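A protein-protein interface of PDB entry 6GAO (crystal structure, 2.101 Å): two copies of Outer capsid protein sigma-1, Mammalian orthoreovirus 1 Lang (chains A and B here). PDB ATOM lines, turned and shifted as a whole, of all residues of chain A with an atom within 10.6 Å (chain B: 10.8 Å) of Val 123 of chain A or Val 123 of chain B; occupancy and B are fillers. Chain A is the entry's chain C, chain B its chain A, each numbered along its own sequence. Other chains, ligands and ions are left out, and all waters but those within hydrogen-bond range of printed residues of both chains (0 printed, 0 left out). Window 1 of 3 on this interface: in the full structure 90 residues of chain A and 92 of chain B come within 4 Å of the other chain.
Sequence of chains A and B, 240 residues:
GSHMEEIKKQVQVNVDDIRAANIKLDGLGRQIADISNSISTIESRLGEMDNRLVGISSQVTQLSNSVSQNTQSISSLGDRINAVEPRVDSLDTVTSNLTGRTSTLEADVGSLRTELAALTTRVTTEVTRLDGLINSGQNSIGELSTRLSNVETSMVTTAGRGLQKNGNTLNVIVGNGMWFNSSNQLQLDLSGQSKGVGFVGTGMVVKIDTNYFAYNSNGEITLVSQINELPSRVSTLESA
Leu 119 of chain B touches its own counterpart, Leu 119 of chain A. Arg 122 of chain A touches Thr 120 of chain B, but with the chains exchanged Thr 120 of chain A does not touch Arg 122 of chain B (11.7 Å). Glu 126 of chain A touches Val 127 of chain B, but with the chains exchanged Val 127 of chain A does not touch Glu 126 of chain B (9.1 Å). Leu 130 of chain A touches Asp 131 of chain B, but with the chains exchanged Asp 131 of chain A does not touch Leu 130 of chain B (8.1 Å). 17 positions are printed for both chains.
The backbone carbonyl oxygen of Thr 124 of chain B sits at hydrogen-bond distance from the side-chain hydroxyl of Thr 128 of chain B (3.0 Å). The backbone carbonyl oxygen (O) of Thr 120 of chain B is in hydrogen-bond range of the side-chain hydroxyl (OG1) of Thr 124 of chain B, at 2.9 Å. The side-chain carboxylate (OE2) of Glu 126 of chain A lies within salt-bridge range of the guanidinium group (NH2) of Arg 129 of chain A. OG1 of Thr 120 of chain B lies within hydrogen-bond range of O of Leu 116 of chain B, 3.0 Å away.
Of chain B, only Leu 116 (3.7 Å), Leu 119 (3.8 Å) and Thr 120 (3.8 Å) come within 4 Å of Leu 119 of chain A. No residue of chain B comes within 4 Å of Thr 120 of chain A. No residue of chain B comes within 4 Å of Thr 121 of chain A. Of chain B, only Thr 120 (3.1 Å), Val 123 (3.6 Å) and Thr 124 (2.7 Å) come within 4 Å of Arg 122 of chain A. Of chain B, only Val 123 comes within 4 Å of Val 123 of chain A. No residue of chain B comes within 4 Å of Thr 125 of chain A. Of the printed residues of chain B, Glu 126 of chain A touches Val 127 (3.9 Å). Of the printed residues of chain A, Leu 116 of chain B touches Glu 115 (3.6 Å) and Leu 119 (3.7 Å). Of chain A, only Leu 119 comes within 4 Å of Leu 119 of chain B. Arg 122 of chain B touches none of the printed residues of chain A. Of the printed residues of chain A, Thr 124 of chain B touches Arg 122. No residue of chain A comes within 4 Å of Thr 125 of chain B. Printed residues of chain A within 4 Å of Val 127 of chain B: Glu 126 and Arg 129. Of the printed residues of chain A, Leu 130 of chain B touches Leu 130. Of the printed residues of chain A, Asp 131 of chain B touches Arg 129 (2.8 Å) and Leu 130 (3.4 Å). The nearest residue of chain B that does not touch Val 123 of chain A is Leu 119 of chain B (6.5 Å). The nearest printed residue of chain B that does not touch Glu 115 of chain A is Thr 120 of chain B (6.3 Å).
NH2 of Arg 122 of chain A sits at hydrogen-bond distance from OG1 of Thr 124 of chain B, 2.7 Å away. The side-chain carboxylate (OD2) of Asp 131 of chain B lies within salt-bridge range of the guanidinium group (NH2) of Arg 129 of chain A (2.8 Å). The backbone carbonyl oxygen (O) of Thr 120 of chain B lies within hydrogen-bond range of the guanidinium group (NH1) of Arg 122 of chain A.
Leu 116 of chain B touches Glu 115 of chain A. CD1 of Leu 116 of chain B touches CD2 of Leu 119 of chain A, 3.7 Å away. CD2 of Leu 119 of chain A touches CD2 of Leu 119 of chain B, at 3.8 Å. Leu 119 of chain A touches Thr 120 of chain B (CD2 to OG1, 3.8 Å). CZ of Arg 122 of chain A touches CG1 of Val 123 of chain B, at 3.6 Å. CG2 of Val 123 of chain B touches CG2 of Val 123 of chain A, at 3.7 Å. Glu 126 of chain A touches Val 127 of chain B (OE2 to CG1, 3.9 Å). NH2 of Arg 129 of chain A touches CG1 of Val 127 of chain B, 3.3 Å away. CD1 of Leu 130 of chain B touches CD1 of Leu 130 of chain A (3.7 Å). CD2 of Leu 130 of chain A touches OD1 of Asp 131 of chain B (3.4 Å).
Of the 17 printed residues of chain B, 8 touch a printed residue of chain A. Hydrophobic or aromatic side chains of chain B within 4 Å of the printed part of chain A: Leu 116, Leu 119, Val 123, Val 127 and Leu 130. Of the 17 printed residues of chain A, 7 touch a printed residue of chain B. Hydrophobic or aromatic side chains of chain A within 4 Å of the printed part of chain B: Leu 119, Val 123 and Leu 130. Among the printed residues, 13 pairs touch across the chains.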
ATOM      1  N   GLU A 115      10.627   5.048  20.270  1.00  0.00           N
ATOM      2  CA  GLU A 115       9.283   5.594  20.174  1.00  0.00           C
ATOM      3  C   GLU A 115       9.307   7.099  19.920  1.00  0.00           C
ATOM      4  O   GLU A 115       8.572   7.605  19.062  1.00  0.00           O
ATOM      5  CB  GLU A 115       8.517   5.232  21.458  1.00  0.00           C
ATOM      6  CG  GLU A 115       8.301   3.692  21.603  1.00  0.00           C
ATOM      7  CD  GLU A 115       8.042   3.242  23.035  1.00  0.00           C
ATOM      8  OE1 GLU A 115       8.405   2.082  23.389  1.00  0.00           O
ATOM      9  OE2 GLU A 115       7.510   4.064  23.814  1.00  0.00           O
ATOM     10  N   LEU A 116      10.170   7.833  20.623  1.00  0.00           N
ATOM     11  CA  LEU A 116      10.251   9.277  20.388  1.00  0.00           C
ATOM     12  C   LEU A 116      10.716   9.597  18.974  1.00  0.00           C
ATOM     13  O   LEU A 116      10.270  10.576  18.373  1.00  0.00           O
ATOM     14  CB  LEU A 116      11.198   9.921  21.380  1.00  0.00           C
ATOM     15  CG  LEU A 116      11.604  11.373  21.264  1.00  0.00           C
ATOM     16  CD1 LEU A 116      10.404  12.253  21.462  1.00  0.00           C
ATOM     17  CD2 LEU A 116      12.688  11.639  22.331  1.00  0.00           C
ATOM     18  N   ALA A 117      11.627   8.799  18.434  1.00  0.00           N
ATOM     19  CA  ALA A 117      12.114   9.063  17.092  1.00  0.00           C
ATOM     20  C   ALA A 117      11.012   8.820  16.071  1.00  0.00           C
ATOM     21  O   ALA A 117      10.878   9.571  15.102  1.00  0.00           O
ATOM     22  CB  ALA A 117      13.333   8.204  16.791  1.00  0.00           C
ATOM     23  N   ALA A 118      10.198   7.791  16.297  1.00  0.00           N
ATOM     24  CA  ALA A 118       9.040   7.554  15.454  1.00  0.00           C
ATOM     25  C   ALA A 118       8.017   8.688  15.599  1.00  0.00           C
ATOM     26  O   ALA A 118       7.456   9.162  14.605  1.00  0.00           O
ATOM     27  CB  ALA A 118       8.423   6.201  15.812  1.00  0.00           C
ATOM     28  N   LEU A 119       7.776   9.158  16.828  1.00  0.00           N
ATOM     29  CA  LEU A 119       6.814  10.241  17.001  1.00  0.00           C
ATOM     30  C   LEU A 119       7.308  11.517  16.335  1.00  0.00           C
ATOM     31  O   LEU A 119       6.514  12.283  15.784  1.00  0.00           O
ATOM     32  CB  LEU A 119       6.546  10.495  18.477  1.00  0.00           C
ATOM     33  CG  LEU A 119       5.523  11.606  18.772  1.00  0.00           C
ATOM     34  CD1 LEU A 119       4.196  11.324  18.056  1.00  0.00           C
ATOM     35  CD2 LEU A 119       5.299  11.789  20.272  1.00  0.00           C
ATOM     36  N   THR A 120       8.618  11.769  16.398  1.00  0.00           N
ATOM     37  CA  THR A 120       9.173  12.940  15.746  1.00  0.00           C
ATOM     38  C   THR A 120       8.947  12.866  14.244  1.00  0.00           C
ATOM     39  O   THR A 120       8.519  13.852  13.635  1.00  0.00           O
ATOM     40  CB  THR A 120      10.652  13.085  16.083  1.00  0.00           C
ATOM     41  OG1 THR A 120      10.789  13.111  17.509  1.00  0.00           O
ATOM     42  CG2 THR A 120      11.225  14.369  15.522  1.00  0.00           C
ATOM     43  N   THR A 121       9.142  11.678  13.659  1.00  0.00           N
ATOM     44  CA  THR A 121       8.890  11.480  12.235  1.00  0.00           C
ATOM     45  C   THR A 121       7.397  11.580  11.897  1.00  0.00           C
ATOM     46  O   THR A 121       7.027  12.101  10.842  1.00  0.00           O
ATOM     47  CB  THR A 121       9.470  10.128  11.823  1.00  0.00           C
ATOM     48  OG1 THR A 121      10.881  10.160  12.064  1.00  0.00           O
ATOM     49  CG2 THR A 121       9.275   9.902  10.347  1.00  0.00           C
ATOM     50  N   ARG A 122       6.531  11.066  12.777  1.00  0.00           N
ATOM     51  CA  ARG A 122       5.092  11.160  12.586  1.00  0.00           C
ATOM     52  C   ARG A 122       4.657  12.609  12.516  1.00  0.00           C
ATOM     53  O   ARG A 122       3.874  12.996  11.637  1.00  0.00           O
ATOM     54  CB  ARG A 122       4.355  10.448  13.723  1.00  0.00           C
ATOM     55  CG  ARG A 122       2.829  10.448  13.564  1.00  0.00           C
ATOM     56  CD  ARG A 122       2.149   9.688  14.703  1.00  0.00           C
ATOM     57  NE  ARG A 122       0.734  10.007  14.687  1.00  0.00           N
ATOM     58  CZ  ARG A 122      -0.054  10.149  15.752  1.00  0.00           C
ATOM     59  NH1 ARG A 122       0.413   9.968  16.997  1.00  0.00           N
ATOM     60  NH2 ARG A 122      -1.345  10.464  15.557  1.00  0.00           N
ATOM     61  N   VAL A 123       5.154  13.425  13.437  1.00  0.00           N
ATOM     62  CA  VAL A 123       4.812  14.840  13.426  1.00  0.00           C
ATOM     63  C   VAL A 123       5.173  15.475  12.080  1.00  0.00           C
ATOM     64  O   VAL A 123       4.358  16.186  11.487  1.00  0.00           O
ATOM     65  CB  VAL A 123       5.486  15.563  14.607  1.00  0.00           C
ATOM     66  CG1 VAL A 123       5.602  17.009  14.325  1.00  0.00           C
ATOM     67  CG2 VAL A 123       4.676  15.338  15.900  1.00  0.00           C
ATOM     68  N   THR A 124       6.384  15.210  11.565  1.00  0.00           N
ATOM     69  CA  THR A 124       6.785  15.775  10.269  1.00  0.00           C
ATOM     70  C   THR A 124       5.885  15.307   9.128  1.00  0.00           C
ATOM     71  O   THR A 124       5.538  16.091   8.232  1.00  0.00           O
ATOM     72  CB  THR A 124       8.226  15.387   9.961  1.00  0.00           C
ATOM     73  OG1 THR A 124       9.080  15.972  10.944  1.00  0.00           O
ATOM     74  CG2 THR A 124       8.606  15.886   8.572  1.00  0.00           C
ATOM     75  N   THR A 125       5.533  14.020   9.137  1.00  0.00           N
ATOM     76  CA  THR A 125       4.700  13.413   8.105  1.00  0.00           C
ATOM     77  C   THR A 125       3.330  14.052   8.052  1.00  0.00           C
ATOM     78  O   THR A 125       2.790  14.306   6.968  1.00  0.00           O
ATOM     79  CB  THR A 125       4.517  11.936   8.412  1.00  0.00           C
ATOM     80  OG1 THR A 125       5.729  11.254   8.157  1.00  0.00           O
ATOM     81  CG2 THR A 125       3.354  11.335   7.572  1.00  0.00           C
ATOM     82  N   GLU A 126       2.730  14.254   9.221  1.00  0.00           N
ATOM     83  CA  GLU A 126       1.364  14.751   9.293  1.00  0.00           C
ATOM     84  C   GLU A 126       1.310  16.240   9.000  1.00  0.00           C
ATOM     85  O   GLU A 126       0.373  16.726   8.354  1.00  0.00           O
ATOM     86  CB  GLU A 126       0.776  14.436  10.669  1.00  0.00           C
ATOM     87  CG  GLU A 126       0.378  12.988  10.902  1.00  0.00           C
ATOM     88  CD  GLU A 126      -0.559  12.385   9.810  1.00  0.00           C
ATOM     89  OE1 GLU A 126      -0.526  11.150   9.662  1.00  0.00           O
ATOM     90  OE2 GLU A 126      -1.300  13.116   9.081  1.00  0.00           O
ATOM     91  N   VAL A 127       2.306  16.983   9.457  1.00  0.00           N
ATOM     92  CA  VAL A 127       2.364  18.399   9.119  1.00  0.00           C
ATOM     93  C   VAL A 127       2.513  18.579   7.617  1.00  0.00           C
ATOM     94  O   VAL A 127       1.844  19.421   7.009  1.00  0.00           O
ATOM     95  CB  VAL A 127       3.507  19.073   9.882  1.00  0.00           C
ATOM     96  CG1 VAL A 127       3.789  20.429   9.250  1.00  0.00           C
ATOM     97  CG2 VAL A 127       3.123  19.192  11.312  1.00  0.00           C
ATOM     98  N   THR A 128       3.352  17.752   6.994  1.00  0.00           N
ATOM     99  CA  THR A 128       3.523  17.760   5.544  1.00  0.00           C
ATOM    100  C   THR A 128       2.212  17.447   4.821  1.00  0.00           C
ATOM    101  O   THR A 128       1.837  18.131   3.856  1.00  0.00           O
ATOM    102  CB  THR A 128       4.598  16.738   5.160  1.00  0.00           C
ATOM    103  OG1 THR A 128       5.835  17.131   5.735  1.00  0.00           O
ATOM    104  CG2 THR A 128       4.755  16.620   3.620  1.00  0.00           C
ATOM    105  N   ARG A 129       1.492  16.419   5.271  1.00  0.00           N
ATOM    106  CA  ARG A 129       0.225  16.110   4.625  1.00  0.00           C
ATOM    107  C   ARG A 129      -0.766  17.259   4.785  1.00  0.00           C
ATOM    108  O   ARG A 129      -1.453  17.626   3.826  1.00  0.00           O
ATOM    109  CB  ARG A 129      -0.354  14.813   5.183  1.00  0.00           C
ATOM    110  CG  ARG A 129      -1.701  14.403   4.546  1.00  0.00           C
ATOM    111  CD  ARG A 129      -2.298  13.101   5.114  1.00  0.00           C
ATOM    112  NE  ARG A 129      -2.592  13.253   6.530  1.00  0.00           N
ATOM    113  CZ  ARG A 129      -3.644  13.906   7.016  1.00  0.00           C
ATOM    114  NH1 ARG A 129      -4.548  14.472   6.206  1.00  0.00           N
ATOM    115  NH2 ARG A 129      -3.775  14.002   8.330  1.00  0.00           N
ATOM    116  N   LEU A 130      -0.852  17.844   5.991  1.00  0.00           N
ATOM    117  CA  LEU A 130      -1.792  18.942   6.244  1.00  0.00           C
ATOM    118  C   LEU A 130      -1.408  20.196   5.461  1.00  0.00           C
ATOM    119  O   LEU A 130      -2.276  20.845   4.851  1.00  0.00           O
ATOM    120  CB  LEU A 130      -1.881  19.246   7.759  1.00  0.00           C
ATOM    121  CG  LEU A 130      -2.482  18.182   8.691  1.00  0.00           C
ATOM    122  CD1 LEU A 130      -2.318  18.526  10.180  1.00  0.00           C
ATOM    123  CD2 LEU A 130      -3.948  17.978   8.425  1.00  0.00           C
ATOM    124  N   ASP A 131      -0.118  20.544   5.439  1.00  0.00           N
ATOM    125  CA  ASP A 131       0.340  21.664   4.603  1.00  0.00           C
ATOM    126  C   ASP A 131      -0.038  21.476   3.139  1.00  0.00           C
ATOM    127  O   ASP A 131      -0.370  22.441   2.459  1.00  0.00           O
ATOM    128  CB  ASP A 131       1.857  21.831   4.697  1.00  0.00           C
ATOM    129  CG  ASP A 131       2.306  22.748   5.840  1.00  0.00           C
ATOM    130  OD1 ASP A 131       1.704  23.819   6.070  1.00  0.00           O
ATOM    131  OD2 ASP A 131       3.298  22.401   6.507  1.00  0.00           O
ATOM    132  N   GLU B 115       4.607  11.134  29.818  1.00  0.00           N
ATOM    133  CA  GLU B 115       4.599  12.318  28.978  1.00  0.00           C
ATOM    134  C   GLU B 115       4.734  11.970  27.495  1.00  0.00           C
ATOM    135  O   GLU B 115       4.251  12.710  26.642  1.00  0.00           O
ATOM    136  CB  GLU B 115       5.715  13.245  29.419  1.00  0.00           C
ATOM    137  CG  GLU B 115       5.440  13.852  30.801  1.00  0.00           C
ATOM    138  CD  GLU B 115       6.698  14.404  31.511  1.00  0.00           C
ATOM    139  OE1 GLU B 115       6.559  14.947  32.641  1.00  0.00           O
ATOM    140  OE2 GLU B 115       7.815  14.303  30.942  1.00  0.00           O
ATOM    141  N   LEU B 116       5.405  10.882  27.150  1.00  0.00           N
ATOM    142  CA  LEU B 116       5.397  10.485  25.752  1.00  0.00           C
ATOM    143  C   LEU B 116       4.020   9.977  25.330  1.00  0.00           C
ATOM    144  O   LEU B 116       3.550  10.310  24.243  1.00  0.00           O
ATOM    145  CB  LEU B 116       6.470   9.428  25.500  1.00  0.00           C
ATOM    146  CG  LEU B 116       6.580   8.996  24.018  1.00  0.00           C
ATOM    147  CD1 LEU B 116       6.930  10.202  23.181  1.00  0.00           C
ATOM    148  CD2 LEU B 116       7.646   7.872  23.792  1.00  0.00           C
ATOM    149  N   ALA B 117       3.356   9.175  26.174  1.00  0.00           N
ATOM    150  CA  ALA B 117       2.065   8.604  25.810  1.00  0.00           C
ATOM    151  C   ALA B 117       1.027   9.690  25.589  1.00  0.00           C
ATOM    152  O   ALA B 117       0.194   9.601  24.670  1.00  0.00           O
ATOM    153  CB  ALA B 117       1.579   7.661  26.902  1.00  0.00           C
ATOM    154  N   ALA B 118       1.040  10.703  26.452  1.00  0.00           N
ATOM    155  CA  ALA B 118       0.112  11.811  26.338  1.00  0.00           C
ATOM    156  C   ALA B 118       0.415  12.655  25.103  1.00  0.00           C
ATOM    157  O   ALA B 118      -0.513  13.148  24.447  1.00  0.00           O
ATOM    158  CB  ALA B 118       0.172  12.657  27.617  1.00  0.00           C
ATOM    159  N   LEU B 119       1.704  12.825  24.759  1.00  0.00           N
ATOM    160  CA  LEU B 119       2.028  13.607  23.565  1.00  0.00           C
ATOM    161  C   LEU B 119       1.615  12.874  22.292  1.00  0.00           C
ATOM    162  O   LEU B 119       1.190  13.514  21.323  1.00  0.00           O
ATOM    163  CB  LEU B 119       3.528  13.957  23.524  1.00  0.00           C
ATOM    164  CG  LEU B 119       3.974  14.796  22.289  1.00  0.00           C
ATOM    165  CD1 LEU B 119       3.255  16.125  22.189  1.00  0.00           C
ATOM    166  CD2 LEU B 119       5.469  15.044  22.298  1.00  0.00           C
ATOM    167  N   THR B 120       1.688  11.531  22.296  1.00  0.00           N
ATOM    168  CA  THR B 120       1.235  10.745  21.150  1.00  0.00           C
ATOM    169  C   THR B 120      -0.258  10.943  20.888  1.00  0.00           C
ATOM    170  O   THR B 120      -0.682  11.044  19.732  1.00  0.00           O
ATOM    171  CB  THR B 120       1.556   9.258  21.366  1.00  0.00           C
ATOM    172  OG1 THR B 120       2.968   9.083  21.597  1.00  0.00           O
ATOM    173  CG2 THR B 120       1.142   8.435  20.138  1.00  0.00           C
ATOM    174  N   THR B 121      -1.076  10.968  21.943  1.00  0.00           N
ATOM    175  CA  THR B 121      -2.510  11.140  21.756  1.00  0.00           C
ATOM    176  C   THR B 121      -2.842  12.560  21.333  1.00  0.00           C
ATOM    177  O   THR B 121      -3.745  12.779  20.520  1.00  0.00           O
ATOM    178  CB  THR B 121      -3.264  10.797  23.037  1.00  0.00           C
ATOM    179  OG1 THR B 121      -2.647  11.479  24.137  1.00  0.00           O
ATOM    180  CG2 THR B 121      -3.237   9.333  23.266  1.00  0.00           C
ATOM    181  N   ARG B 122      -2.141  13.527  21.907  1.00  0.00           N
ATOM    182  CA  ARG B 122      -2.251  14.913  21.501  1.00  0.00           C
ATOM    183  C   ARG B 122      -2.018  15.081  20.009  1.00  0.00           C
ATOM    184  O   ARG B 122      -2.745  15.841  19.350  1.00  0.00           O
ATOM    185  CB  ARG B 122      -1.247  15.770  22.284  1.00  0.00           C
ATOM    186  CG  ARG B 122      -1.342  17.257  21.944  1.00  0.00           C
ATOM    187  CD  ARG B 122      -0.404  18.143  22.752  1.00  0.00           C
ATOM    188  NE  ARG B 122      -0.454  19.515  22.245  1.00  0.00           N
ATOM    189  CZ  ARG B 122       0.589  20.332  22.213  1.00  0.00           C
ATOM    190  NH1 ARG B 122       1.779  19.924  22.667  1.00  0.00           N
ATOM    191  NH2 ARG B 122       0.461  21.553  21.722  1.00  0.00           N
ATOM    192  N   VAL B 123      -0.990  14.422  19.463  1.00  0.00           N
ATOM    193  CA  VAL B 123      -0.706  14.563  18.039  1.00  0.00           C
ATOM    194  C   VAL B 123      -1.901  14.064  17.207  1.00  0.00           C
ATOM    195  O   VAL B 123      -2.344  14.740  16.280  1.00  0.00           O
ATOM    196  CB  VAL B 123       0.612  13.852  17.672  1.00  0.00           C
ATOM    197  CG1 VAL B 123       0.729  13.684  16.148  1.00  0.00           C
ATOM    198  CG2 VAL B 123       1.768  14.698  18.134  1.00  0.00           C
ATOM    199  N   THR B 124      -2.494  12.929  17.597  1.00  0.00           N
ATOM    200  CA  THR B 124      -3.656  12.350  16.903  1.00  0.00           C
ATOM    201  C   THR B 124      -4.877  13.255  16.968  1.00  0.00           C
ATOM    202  O   THR B 124      -5.583  13.464  15.962  1.00  0.00           O
ATOM    203  CB  THR B 124      -3.994  11.018  17.560  1.00  0.00           C
ATOM    204  OG1 THR B 124      -2.774  10.345  17.858  1.00  0.00           O
ATOM    205  CG2 THR B 124      -4.869  10.135  16.675  1.00  0.00           C
ATOM    206  N   THR B 125      -5.186  13.714  18.181  1.00  0.00           N
ATOM    207  CA  THR B 125      -6.295  14.625  18.452  1.00  0.00           C
ATOM    208  C   THR B 125      -6.216  15.861  17.575  1.00  0.00           C
ATOM    209  O   THR B 125      -7.185  16.232  16.923  1.00  0.00           O
ATOM    210  CB  THR B 125      -6.224  15.022  19.943  1.00  0.00           C
ATOM    211  OG1 THR B 125      -6.411  13.862  20.759  1.00  0.00           O
ATOM    212  CG2 THR B 125      -7.210  16.141  20.307  1.00  0.00           C
ATOM    213  N   GLU B 126      -5.051  16.512  17.546  1.00  0.00           N
ATOM    214  CA  GLU B 126      -4.929  17.779  16.833  1.00  0.00           C
ATOM    215  C   GLU B 126      -4.927  17.580  15.320  1.00  0.00           C
ATOM    216  O   GLU B 126      -5.534  18.368  14.592  1.00  0.00           O
ATOM    217  CB  GLU B 126      -3.685  18.512  17.303  1.00  0.00           C
ATOM    218  CG  GLU B 126      -3.787  18.958  18.763  1.00  0.00           C
ATOM    219  CD  GLU B 126      -4.897  19.976  19.009  1.00  0.00           C
ATOM    220  OE1 GLU B 126      -5.614  19.904  20.039  1.00  0.00           O
ATOM    221  OE2 GLU B 126      -5.056  20.851  18.170  1.00  0.00           O
ATOM    222  N   VAL B 127      -4.282  16.524  14.829  1.00  0.00           N
ATOM    223  CA  VAL B 127      -4.376  16.211  13.408  1.00  0.00           C
ATOM    224  C   VAL B 127      -5.829  16.026  13.007  1.00  0.00           C
ATOM    225  O   VAL B 127      -6.326  16.704  12.098  1.00  0.00           O
ATOM    226  CB  VAL B 127      -3.544  14.967  13.060  1.00  0.00           C
ATOM    227  CG1 VAL B 127      -3.884  14.518  11.608  1.00  0.00           C
ATOM    228  CG2 VAL B 127      -2.056  15.255  13.266  1.00  0.00           C
ATOM    229  N   THR B 128      -6.542  15.122  13.689  1.00  0.00           N
ATOM    230  CA  THR B 128      -7.968  14.954  13.425  1.00  0.00           C
ATOM    231  C   THR B 128      -8.722  16.289  13.459  1.00  0.00           C
ATOM    232  O   THR B 128      -9.552  16.563  12.580  1.00  0.00           O
ATOM    233  CB  THR B 128      -8.592  13.990  14.428  1.00  0.00           C
ATOM    234  OG1 THR B 128      -7.992  12.701  14.297  1.00  0.00           O
ATOM    235  CG2 THR B 128     -10.121  13.866  14.182  1.00  0.00           C
ATOM    236  N   ARG B 129      -8.437  17.145  14.451  1.00  0.00           N
ATOM    237  CA  ARG B 129      -9.116  18.437  14.492  1.00  0.00           C
ATOM    238  C   ARG B 129      -8.783  19.266  13.262  1.00  0.00           C
ATOM    239  O   ARG B 129      -9.673  19.890  12.660  1.00  0.00           O
ATOM    240  CB  ARG B 129      -8.764  19.231  15.758  1.00  0.00           C
ATOM    241  CG  ARG B 129      -9.660  20.508  15.920  1.00  0.00           C
ATOM    242  CD  ARG B 129      -9.297  21.344  17.184  1.00  0.00           C
ATOM    243  NE  ARG B 129      -7.881  21.718  17.145  1.00  0.00           N
ATOM    244  CZ  ARG B 129      -7.371  22.713  16.414  1.00  0.00           C
ATOM    245  NH1 ARG B 129      -8.147  23.487  15.655  1.00  0.00           N
ATOM    246  NH2 ARG B 129      -6.076  22.946  16.444  1.00  0.00           N
ATOM    247  N   LEU B 130      -7.513  19.301  12.875  1.00  0.00           N
ATOM    248  CA  LEU B 130      -7.150  20.165  11.759  1.00  0.00           C
ATOM    249  C   LEU B 130      -7.665  19.617  10.430  1.00  0.00           C
ATOM    250  O   LEU B 130      -7.963  20.393   9.528  1.00  0.00           O
ATOM    251  CB  LEU B 130      -5.640  20.345  11.714  1.00  0.00           C
ATOM    252  CG  LEU B 130      -4.967  21.021  12.918  1.00  0.00           C
ATOM    253  CD1 LEU B 130      -3.452  20.898  12.795  1.00  0.00           C
ATOM    254  CD2 LEU B 130      -5.351  22.487  12.946  1.00  0.00           C
ATOM    255  N   ASP B 131      -7.778  18.297  10.288  1.00  0.00           N
ATOM    256  CA  ASP B 131      -8.415  17.745   9.095  1.00  0.00           C
ATOM    257  C   ASP B 131      -9.874  18.172   9.010  1.00  0.00           C
ATOM    258  O   ASP B 131     -10.378  18.469   7.924  1.00  0.00           O
ATOM    259  CB  ASP B 131      -8.317  16.219   9.094  1.00  0.00           C
ATOM    260  CG  ASP B 131      -6.975  15.699   8.523  1.00  0.00           C
ATOM    261  OD1 ASP B 131      -6.589  16.140   7.407  1.00  0.00           O
ATOM    262  OD2 ASP B 131      -6.313  14.857   9.184  1.00  0.00           O
